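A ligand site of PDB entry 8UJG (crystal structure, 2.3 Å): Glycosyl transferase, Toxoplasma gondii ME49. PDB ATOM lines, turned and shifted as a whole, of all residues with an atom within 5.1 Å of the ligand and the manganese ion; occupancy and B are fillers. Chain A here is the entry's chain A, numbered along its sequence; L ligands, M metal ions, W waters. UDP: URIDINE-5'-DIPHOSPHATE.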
ATOM      1  N   VAL A 114      19.094 -13.006   6.243  1.00  0.00           N
ATOM      2  CA  VAL A 114      18.273 -12.640   5.104  1.00  0.00           C
ATOM      3  C   VAL A 114      19.160 -11.977   4.063  1.00  0.00           C
ATOM      4  O   VAL A 114      20.177 -11.345   4.400  1.00  0.00           O
ATOM      5  CB  VAL A 114      17.103 -11.722   5.517  1.00  0.00           C
ATOM      6  CG1 VAL A 114      16.398 -12.288   6.744  1.00  0.00           C
ATOM      7  CG2 VAL A 114      17.595 -10.313   5.789  1.00  0.00           C
ATOM      8  N   PHE A 115      18.795 -12.117   2.794  1.00  0.00           N
ATOM      9  CA  PHE A 115      19.620 -11.592   1.723  1.00  0.00           C
ATOM     10  C   PHE A 115      18.763 -11.357   0.489  1.00  0.00           C
ATOM     11  O   PHE A 115      17.856 -12.139   0.196  1.00  0.00           O
ATOM     12  CB  PHE A 115      20.757 -12.561   1.383  1.00  0.00           C
ATOM     13  CG  PHE A 115      20.292 -13.913   0.936  1.00  0.00           C
ATOM     14  CD1 PHE A 115      19.986 -14.901   1.871  1.00  0.00           C
ATOM     15  CD2 PHE A 115      20.164 -14.213  -0.404  1.00  0.00           C
ATOM     16  CE1 PHE A 115      19.559 -16.144   1.458  1.00  0.00           C
ATOM     17  CE2 PHE A 115      19.735 -15.465  -0.820  1.00  0.00           C
ATOM     18  CZ  PHE A 115      19.437 -16.432   0.113  1.00  0.00           C
ATOM     19  N   TYR A 116      19.060 -10.280  -0.235  1.00  0.00           N
ATOM     20  CA  TYR A 116      18.493 -10.006  -1.554  1.00  0.00           C
ATOM     21  C   TYR A 116      19.652  -9.816  -2.518  1.00  0.00           C
ATOM     22  O   TYR A 116      20.337  -8.789  -2.485  1.00  0.00           O
ATOM     23  CB  TYR A 116      17.572  -8.785  -1.536  1.00  0.00           C
ATOM     24  CG  TYR A 116      17.097  -8.379  -2.915  1.00  0.00           C
ATOM     25  CD1 TYR A 116      16.188  -9.156  -3.612  1.00  0.00           C
ATOM     26  CD2 TYR A 116      17.559  -7.214  -3.508  1.00  0.00           C
ATOM     27  CE1 TYR A 116      15.755  -8.793  -4.871  1.00  0.00           C
ATOM     28  CE2 TYR A 116      17.132  -6.840  -4.773  1.00  0.00           C
ATOM     29  CZ  TYR A 116      16.228  -7.639  -5.441  1.00  0.00           C
ATOM     30  OH  TYR A 116      15.786  -7.273  -6.702  1.00  0.00           O
ATOM     31  N   GLU A 118      22.532 -11.261  -2.665  1.00  0.00           N
ATOM     32  CA  GLU A 118      23.873 -11.310  -2.101  1.00  0.00           C
ATOM     33  C   GLU A 118      24.718 -12.294  -2.902  1.00  0.00           C
ATOM     34  O   GLU A 118      24.293 -13.435  -3.118  1.00  0.00           O
ATOM     35  CB  GLU A 118      23.830 -11.727  -0.630  1.00  0.00           C
ATOM     36  CG  GLU A 118      25.189 -11.647   0.077  1.00  0.00           C
ATOM     37  CD  GLU A 118      25.620 -10.223   0.347  1.00  0.00           C
ATOM     38  OE1 GLU A 118      24.789  -9.444   0.865  1.00  0.00           O
ATOM     39  OE2 GLU A 118      26.776  -9.875   0.031  1.00  0.00           O
ATOM     40  N   ASP A 147      14.995 -13.178   0.032  1.00  0.00           N
ATOM     41  CA  ASP A 147      13.957 -12.156  -0.076  1.00  0.00           C
ATOM     42  C   ASP A 147      13.697 -11.792  -1.539  1.00  0.00           C
ATOM     43  O   ASP A 147      13.911 -10.677  -1.986  1.00  0.00           O
ATOM     44  CB  ASP A 147      14.350 -10.930   0.733  1.00  0.00           C
ATOM     45  CG  ASP A 147      13.234  -9.906   0.816  1.00  0.00           C
ATOM     46  OD1 ASP A 147      12.060 -10.296   0.697  1.00  0.00           O
ATOM     47  OD2 ASP A 147      13.545  -8.706   0.974  1.00  0.00           O
ATOM     48  N   ARG A 181      10.044  -9.951  -3.334  1.00  0.00           N
ATOM     49  CA  ARG A 181      10.862  -9.195  -2.400  1.00  0.00           C
ATOM     50  C   ARG A 181       9.975  -8.397  -1.452  1.00  0.00           C
ATOM     51  O   ARG A 181       9.162  -7.578  -1.895  1.00  0.00           O
ATOM     52  CB  ARG A 181      11.785  -8.251  -3.161  1.00  0.00           C
ATOM     53  CG  ARG A 181      12.586  -7.310  -2.277  1.00  0.00           C
ATOM     54  CD  ARG A 181      13.397  -6.338  -3.103  1.00  0.00           C
ATOM     55  NE  ARG A 181      14.108  -5.381  -2.266  1.00  0.00           N
ATOM     56  CZ  ARG A 181      14.718  -4.299  -2.726  1.00  0.00           C
ATOM     57  NH1 ARG A 181      14.682  -3.976  -4.009  1.00  0.00           N
ATOM     58  NH2 ARG A 181      15.363  -3.508  -1.871  1.00  0.00           N
ATOM     59  N   GLY A 183      11.420  -6.871   1.571  1.00  0.00           N
ATOM     60  CA  GLY A 183      12.234  -5.880   2.249  1.00  0.00           C
ATOM     61  C   GLY A 183      12.863  -6.442   3.510  1.00  0.00           C
ATOM     62  O   GLY A 183      12.671  -7.609   3.875  1.00  0.00           O
ATOM     63  N   ILE A 184      13.620  -5.579   4.185  1.00  0.00           N
ATOM     64  CA  ILE A 184      14.351  -5.995   5.371  1.00  0.00           C
ATOM     65  C   ILE A 184      13.394  -6.511   6.442  1.00  0.00           C
ATOM     66  O   ILE A 184      13.580  -7.595   6.997  1.00  0.00           O
ATOM     67  CB  ILE A 184      15.221  -4.834   5.904  1.00  0.00           C
ATOM     68  CG1 ILE A 184      16.558  -4.808   5.157  1.00  0.00           C
ATOM     69  CG2 ILE A 184      15.447  -4.967   7.412  1.00  0.00           C
ATOM     70  CD1 ILE A 184      17.441  -3.621   5.489  1.00  0.00           C
ATOM     71  N   ALA A 187      11.526  -9.700   5.296  1.00  0.00           N
ATOM     72  CA  ALA A 187      12.432 -10.840   5.213  1.00  0.00           C
ATOM     73  C   ALA A 187      12.800 -11.353   6.596  1.00  0.00           C
ATOM     74  O   ALA A 187      12.805 -12.563   6.835  1.00  0.00           O
ATOM     75  CB  ALA A 187      13.697 -10.450   4.439  1.00  0.00           C
ATOM     76  N   ARG A 188      13.102 -10.444   7.529  1.00  0.00           N
ATOM     77  CA  ARG A 188      13.480 -10.879   8.869  1.00  0.00           C
ATOM     78  C   ARG A 188      12.316 -11.527   9.598  1.00  0.00           C
ATOM     79  O   ARG A 188      12.500 -12.526  10.310  1.00  0.00           O
ATOM     80  CB  ARG A 188      14.007  -9.692   9.671  1.00  0.00           C
ATOM     81  CG  ARG A 188      15.358  -9.195   9.177  1.00  0.00           C
ATOM     82  CD  ARG A 188      15.850  -8.003   9.988  1.00  0.00           C
ATOM     83  NE  ARG A 188      17.097  -7.481   9.432  1.00  0.00           N
ATOM     84  CZ  ARG A 188      17.586  -6.274   9.694  1.00  0.00           C
ATOM     85  NH1 ARG A 188      16.967  -5.433  10.502  1.00  0.00           N
ATOM     86  NH2 ARG A 188      18.725  -5.908   9.127  1.00  0.00           N
ATOM     87  N   ASP A 204      23.889 -10.015   9.084  1.00  0.00           N
ATOM     88  CA  ASP A 204      23.891  -9.637   7.686  1.00  0.00           C
ATOM     89  C   ASP A 204      24.474 -10.772   6.840  1.00  0.00           C
ATOM     90  O   ASP A 204      25.111 -11.697   7.358  1.00  0.00           O
ATOM     91  CB  ASP A 204      24.685  -8.353   7.451  1.00  0.00           C
ATOM     92  CG  ASP A 204      23.877  -7.099   7.754  1.00  0.00           C
ATOM     93  OD1 ASP A 204      22.846  -7.222   8.454  1.00  0.00           O
ATOM     94  OD2 ASP A 204      24.277  -6.010   7.292  1.00  0.00           O
ATOM     95  N   SER A 205      24.272 -10.686   5.534  1.00  0.00           N
ATOM     96  CA  SER A 205      24.709 -11.714   4.607  1.00  0.00           C
ATOM     97  C   SER A 205      26.121 -11.481   4.083  1.00  0.00           C
ATOM     98  O   SER A 205      26.517 -12.080   3.079  1.00  0.00           O
ATOM     99  CB  SER A 205      23.723 -11.808   3.433  1.00  0.00           C
ATOM    100  OG  SER A 205      23.541 -10.552   2.822  1.00  0.00           O
ATOM    101  N   HIS A 206      26.892 -10.602   4.734  1.00  0.00           N
ATOM    102  CA  HIS A 206      28.257 -10.268   4.351  1.00  0.00           C
ATOM    103  C   HIS A 206      29.048  -9.992   5.631  1.00  0.00           C
ATOM    104  O   HIS A 206      29.472  -8.878   5.919  1.00  0.00           O
ATOM    105  CB  HIS A 206      28.279  -9.073   3.387  1.00  0.00           C
ATOM    106  CG  HIS A 206      27.220  -8.052   3.686  1.00  0.00           C
ATOM    107  ND1 HIS A 206      26.065  -7.947   2.939  1.00  0.00           N
ATOM    108  CD2 HIS A 206      27.143  -7.093   4.633  1.00  0.00           C
ATOM    109  CE1 HIS A 206      25.316  -6.978   3.419  1.00  0.00           C
ATOM    110  NE2 HIS A 206      25.945  -6.432   4.450  1.00  0.00           N
ATOM    111  N   PHE A 313      10.722  -1.942   2.214  1.00  0.00           N
ATOM    112  CA  PHE A 313      12.050  -2.159   1.660  1.00  0.00           C
ATOM    113  C   PHE A 313      13.133  -1.889   2.709  1.00  0.00           C
ATOM    114  O   PHE A 313      13.282  -2.676   3.640  1.00  0.00           O
ATOM    115  CB  PHE A 313      12.224  -1.287   0.410  1.00  0.00           C
ATOM    116  CG  PHE A 313      11.358  -1.718  -0.753  1.00  0.00           C
ATOM    117  CD1 PHE A 313      11.727  -2.802  -1.545  1.00  0.00           C
ATOM    118  CD2 PHE A 313      10.173  -1.064  -1.045  1.00  0.00           C
ATOM    119  CE1 PHE A 313      10.933  -3.212  -2.603  1.00  0.00           C
ATOM    120  CE2 PHE A 313       9.385  -1.463  -2.108  1.00  0.00           C
ATOM    121  CZ  PHE A 313       9.762  -2.542  -2.885  1.00  0.00           C
ATOM    122  N   TRP A 314      13.879  -0.793   2.573  1.00  0.00           N
ATOM    123  CA  TRP A 314      15.084  -0.565   3.362  1.00  0.00           C
ATOM    124  C   TRP A 314      14.970   0.706   4.193  1.00  0.00           C
ATOM    125  O   TRP A 314      14.441   1.722   3.714  1.00  0.00           O
ATOM    126  CB  TRP A 314      16.319  -0.488   2.448  1.00  0.00           C
ATOM    127  CG  TRP A 314      17.620  -0.311   3.165  1.00  0.00           C
ATOM    128  CD1 TRP A 314      18.511  -1.304   3.497  1.00  0.00           C
ATOM    129  CD2 TRP A 314      18.192   0.906   3.647  1.00  0.00           C
ATOM    130  NE1 TRP A 314      19.595  -0.761   4.156  1.00  0.00           N
ATOM    131  CE2 TRP A 314      19.420   0.593   4.260  1.00  0.00           C
ATOM    132  CE3 TRP A 314      17.778   2.244   3.618  1.00  0.00           C
ATOM    133  CZ2 TRP A 314      20.234   1.553   4.840  1.00  0.00           C
ATOM    134  CZ3 TRP A 314      18.593   3.204   4.198  1.00  0.00           C
ATOM    135  CH2 TRP A 314      19.812   2.855   4.798  1.00  0.00           C
ATOM    136  N   HIS A 342      31.860  -6.892   9.472  1.00  0.00           N
ATOM    137  CA  HIS A 342      30.809  -6.518   8.548  1.00  0.00           C
ATOM    138  C   HIS A 342      31.400  -5.725   7.397  1.00  0.00           C
ATOM    139  O   HIS A 342      32.210  -4.826   7.610  1.00  0.00           O
ATOM    140  CB  HIS A 342      29.719  -5.690   9.244  1.00  0.00           C
ATOM    141  CG  HIS A 342      28.663  -5.174   8.321  1.00  0.00           C
ATOM    142  ND1 HIS A 342      28.758  -3.959   7.678  1.00  0.00           N
ATOM    143  CD2 HIS A 342      27.475  -5.697   7.947  1.00  0.00           C
ATOM    144  CE1 HIS A 342      27.676  -3.766   6.941  1.00  0.00           C
ATOM    145  NE2 HIS A 342      26.881  -4.808   7.080  1.00  0.00           N
ATOM    146  N   ILE A 343      31.002  -6.069   6.173  1.00  0.00           N
ATOM    147  CA  ILE A 343      31.428  -5.334   4.990  1.00  0.00           C
ATOM    148  C   ILE A 343      30.542  -4.100   4.858  1.00  0.00           C
ATOM    149  O   ILE A 343      29.343  -4.212   4.586  1.00  0.00           O
ATOM    150  CB  ILE A 343      31.370  -6.201   3.726  1.00  0.00           C
ATOM    151  CG1 ILE A 343      32.197  -7.476   3.887  1.00  0.00           C
ATOM    152  CG2 ILE A 343      31.868  -5.410   2.521  1.00  0.00           C
ATOM    153  CD1 ILE A 343      32.054  -8.448   2.726  1.00  0.00           C
ATOM    154  N   ARG A 345      29.586  -1.017   2.598  1.00  0.00           N
ATOM    155  CA  ARG A 345      29.739  -0.815   1.166  1.00  0.00           C
ATOM    156  C   ARG A 345      30.427   0.517   0.896  1.00  0.00           C
ATOM    157  O   ARG A 345      30.323   1.472   1.661  1.00  0.00           O
ATOM    158  CB  ARG A 345      28.375  -0.833   0.473  1.00  0.00           C
ATOM    159  CG  ARG A 345      27.549  -2.056   0.799  1.00  0.00           C
ATOM    160  CD  ARG A 345      26.220  -2.078   0.064  1.00  0.00           C
ATOM    161  NE  ARG A 345      25.285  -3.003   0.689  1.00  0.00           N
ATOM    162  CZ  ARG A 345      25.060  -4.232   0.258  1.00  0.00           C
ATOM    163  NH1 ARG A 345      25.825  -4.791  -0.671  1.00  0.00           N
ATOM    164  NH2 ARG A 345      24.091  -4.948   0.810  1.00  0.00           N
ATOM    165  N   TYR A 351      21.600  -3.178  -4.222  1.00  0.00           N
ATOM    166  CA  TYR A 351      20.219  -3.193  -4.674  1.00  0.00           C
ATOM    167  C   TYR A 351      19.676  -1.774  -4.604  1.00  0.00           C
ATOM    168  O   TYR A 351      20.214  -0.927  -3.896  1.00  0.00           O
ATOM    169  CB  TYR A 351      19.354  -4.131  -3.819  1.00  0.00           C
ATOM    170  CG  TYR A 351      19.520  -3.894  -2.332  1.00  0.00           C
ATOM    171  CD1 TYR A 351      18.816  -2.887  -1.687  1.00  0.00           C
ATOM    172  CD2 TYR A 351      20.390  -4.671  -1.593  1.00  0.00           C
ATOM    173  CE1 TYR A 351      18.968  -2.663  -0.334  1.00  0.00           C
ATOM    174  CE2 TYR A 351      20.551  -4.450  -0.237  1.00  0.00           C
ATOM    175  CZ  TYR A 351      19.838  -3.456   0.389  1.00  0.00           C
ATOM    176  OH  TYR A 351      20.001  -3.242   1.734  1.00  0.00           O
HETATM  177  N1  UDP L   1      18.091  -7.193   2.498  1.00  0.00           N
HETATM  178  C2  UDP L   1      17.022  -7.990   2.140  1.00  0.00           C
HETATM  179  N3  UDP L   1      16.031  -7.361   1.433  1.00  0.00           N
HETATM  180  C4  UDP L   1      16.009  -6.029   1.049  1.00  0.00           C
HETATM  181  C5  UDP L   1      17.156  -5.271   1.466  1.00  0.00           C
HETATM  182  C6  UDP L   1      18.143  -5.862   2.159  1.00  0.00           C
HETATM  183  O2  UDP L   1      16.950  -9.179   2.429  1.00  0.00           O
HETATM  184  O4  UDP L   1      15.049  -5.593   0.407  1.00  0.00           O
HETATM  185  C1' UDP L   1      19.186  -7.815   3.265  1.00  0.00           C
HETATM  186  C2' UDP L   1      20.578  -7.504   2.718  1.00  0.00           C
HETATM  187  O2' UDP L   1      20.949  -8.422   1.711  1.00  0.00           O
HETATM  188  C3' UDP L   1      21.435  -7.659   3.973  1.00  0.00           C
HETATM  189  C4' UDP L   1      20.511  -7.166   5.095  1.00  0.00           C
HETATM  190  O4' UDP L   1      19.165  -7.298   4.583  1.00  0.00           O
HETATM  191  O3' UDP L   1      21.824  -9.006   4.191  1.00  0.00           O
HETATM  192  C5' UDP L   1      20.757  -5.741   5.542  1.00  0.00           C
HETATM  193  O5' UDP L   1      20.934  -4.884   4.392  1.00  0.00           O
HETATM  194  PA  UDP L   1      22.269  -4.054   4.190  1.00  0.00           P
HETATM  195  O1A UDP L   1      23.399  -4.964   4.470  1.00  0.00           O
HETATM  196  O2A UDP L   1      22.262  -3.344   2.841  1.00  0.00           O
HETATM  197  O3A UDP L   1      22.190  -2.913   5.296  1.00  0.00           O
HETATM  198  PB  UDP L   1      23.385  -1.909   5.573  1.00  0.00           P
HETATM  199  O1B UDP L   1      22.697  -0.749   6.299  1.00  0.00           O
HETATM  200  O2B UDP L   1      24.273  -2.687   6.545  1.00  0.00           O
HETATM  201  O3B UDP L   1      24.078  -1.502   4.311  1.00  0.00           O
HETATM  202 MN    MN M   1      25.117  -4.768   5.705  1.00  0.00          MN
HETATM  203  O   HOH W   1      26.282  -3.458   4.383  1.00  0.00           O
HETATM  204  O   HOH W   2      22.962  -7.644  -0.339  1.00  0.00           O
HETATM  205  O   HOH W   3      20.642 -10.415   7.112  1.00  0.00           O
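The backbone NH (N) of Gly 183 sits at hydrogen-bond distance from the side-chain carboxylate (OD2) of Asp 147, at 2.9 Å. N of Asp 147 is in hydrogen-bond range of O of Phe 115, at 3.0 Å. The side-chain hydroxyl (OH) of Tyr 351 lies close to the indole nitrogen (NE1) of Trp 314 (3.5 Å). N of Ile 184 sits at hydrogen-bond distance from O of Phe 313, at 3.0 Å. The side-chain hydroxyl of Ser 205 is in hydrogen-bond range of the side-chain carboxylate of Glu 118 (2.6 Å). A ring nitrogen (ND1) of His 206 sits at hydrogen-bond distance from the side-chain carboxylate of Glu 118 (2.9 Å). N of Ile 343 sits at hydrogen-bond distance from O of His 206, 3.2 Å away.
The manganese ion is bound by O1A of the ligand (2.1 Å), OD2 of Asp 204 (2.2 Å), water W1 (2.2 Å), NE2 of His 342 (2.2 Å), NE2 of His 206 (2.2 Å) and O2B of the ligand (2.4 Å).
The side-chain hydroxyl (OH) of Tyr 351 lies within hydrogen-bond range of an oxygen (O2A) of the ligand (2.5 Å). O of Val 114 lies within hydrogen-bond range of O3' of the ligand (2.9 Å). The backbone NH (N) of Ser 205 sits at hydrogen-bond distance from an oxygen (O3') of the ligand, 3.3 Å away. The side-chain carboxylate (OD2) of Asp 147 is in hydrogen-bond range of a nitrogen (N3) of the ligand. An oxygen (O2) of the ligand lies close to the backbone NH of Phe 115, at 3.5 Å. OG of Ser 205 lies within hydrogen-bond range of O3' of the ligand. The guanidinium group (NE) of Arg 181 sits at hydrogen-bond distance from an oxygen (O4) of the ligand (2.8 Å). The guanidinium group (NH2) of Arg 345 lies within salt-bridge range of an oxygen (O2A) of the ligand (3.2 Å). The backbone NH of Tyr 116 lies within hydrogen-bond range of an oxygen (O2') of the ligand (3.3 Å).
Gly 183 touches the ligand (CA to O4, 3.4 Å). Ile 184 touches the ligand. Trp 314 touches the ligand (NE1 to O3A, 3.6 Å). Hydrophobic or aromatic side chains within 4 Å of the ligand: Val 114, Tyr 116, Ile 184, His 206, Trp 314, His 342 and Tyr 351. 14 residues have an atom within 4 Å of the ligand: Val 114, Phe 115, Tyr 116, Asp 147, Arg 181, Gly 183, Ile 184, Asp 204, Ser 205, His 206, Trp 314, His 342, Arg 345 and Tyr 351.
Of the 19 residues printed, 3 come within 4 Å of the manganese ion. The nearest printed residue that does not touch the manganese ion is Ile 343 (4.4 Å).
Water W1 lies within hydrogen-bond range of O3B of the ligand and O of Ile 343. Water W2 lies within hydrogen-bond range of the side-chain carboxylate (OE1) of Glu 118, an oxygen (O2') of the ligand and the guanidinium group (NH2) of Arg 345. Water W3 bridges O of Val 114 and O3' of the ligand.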
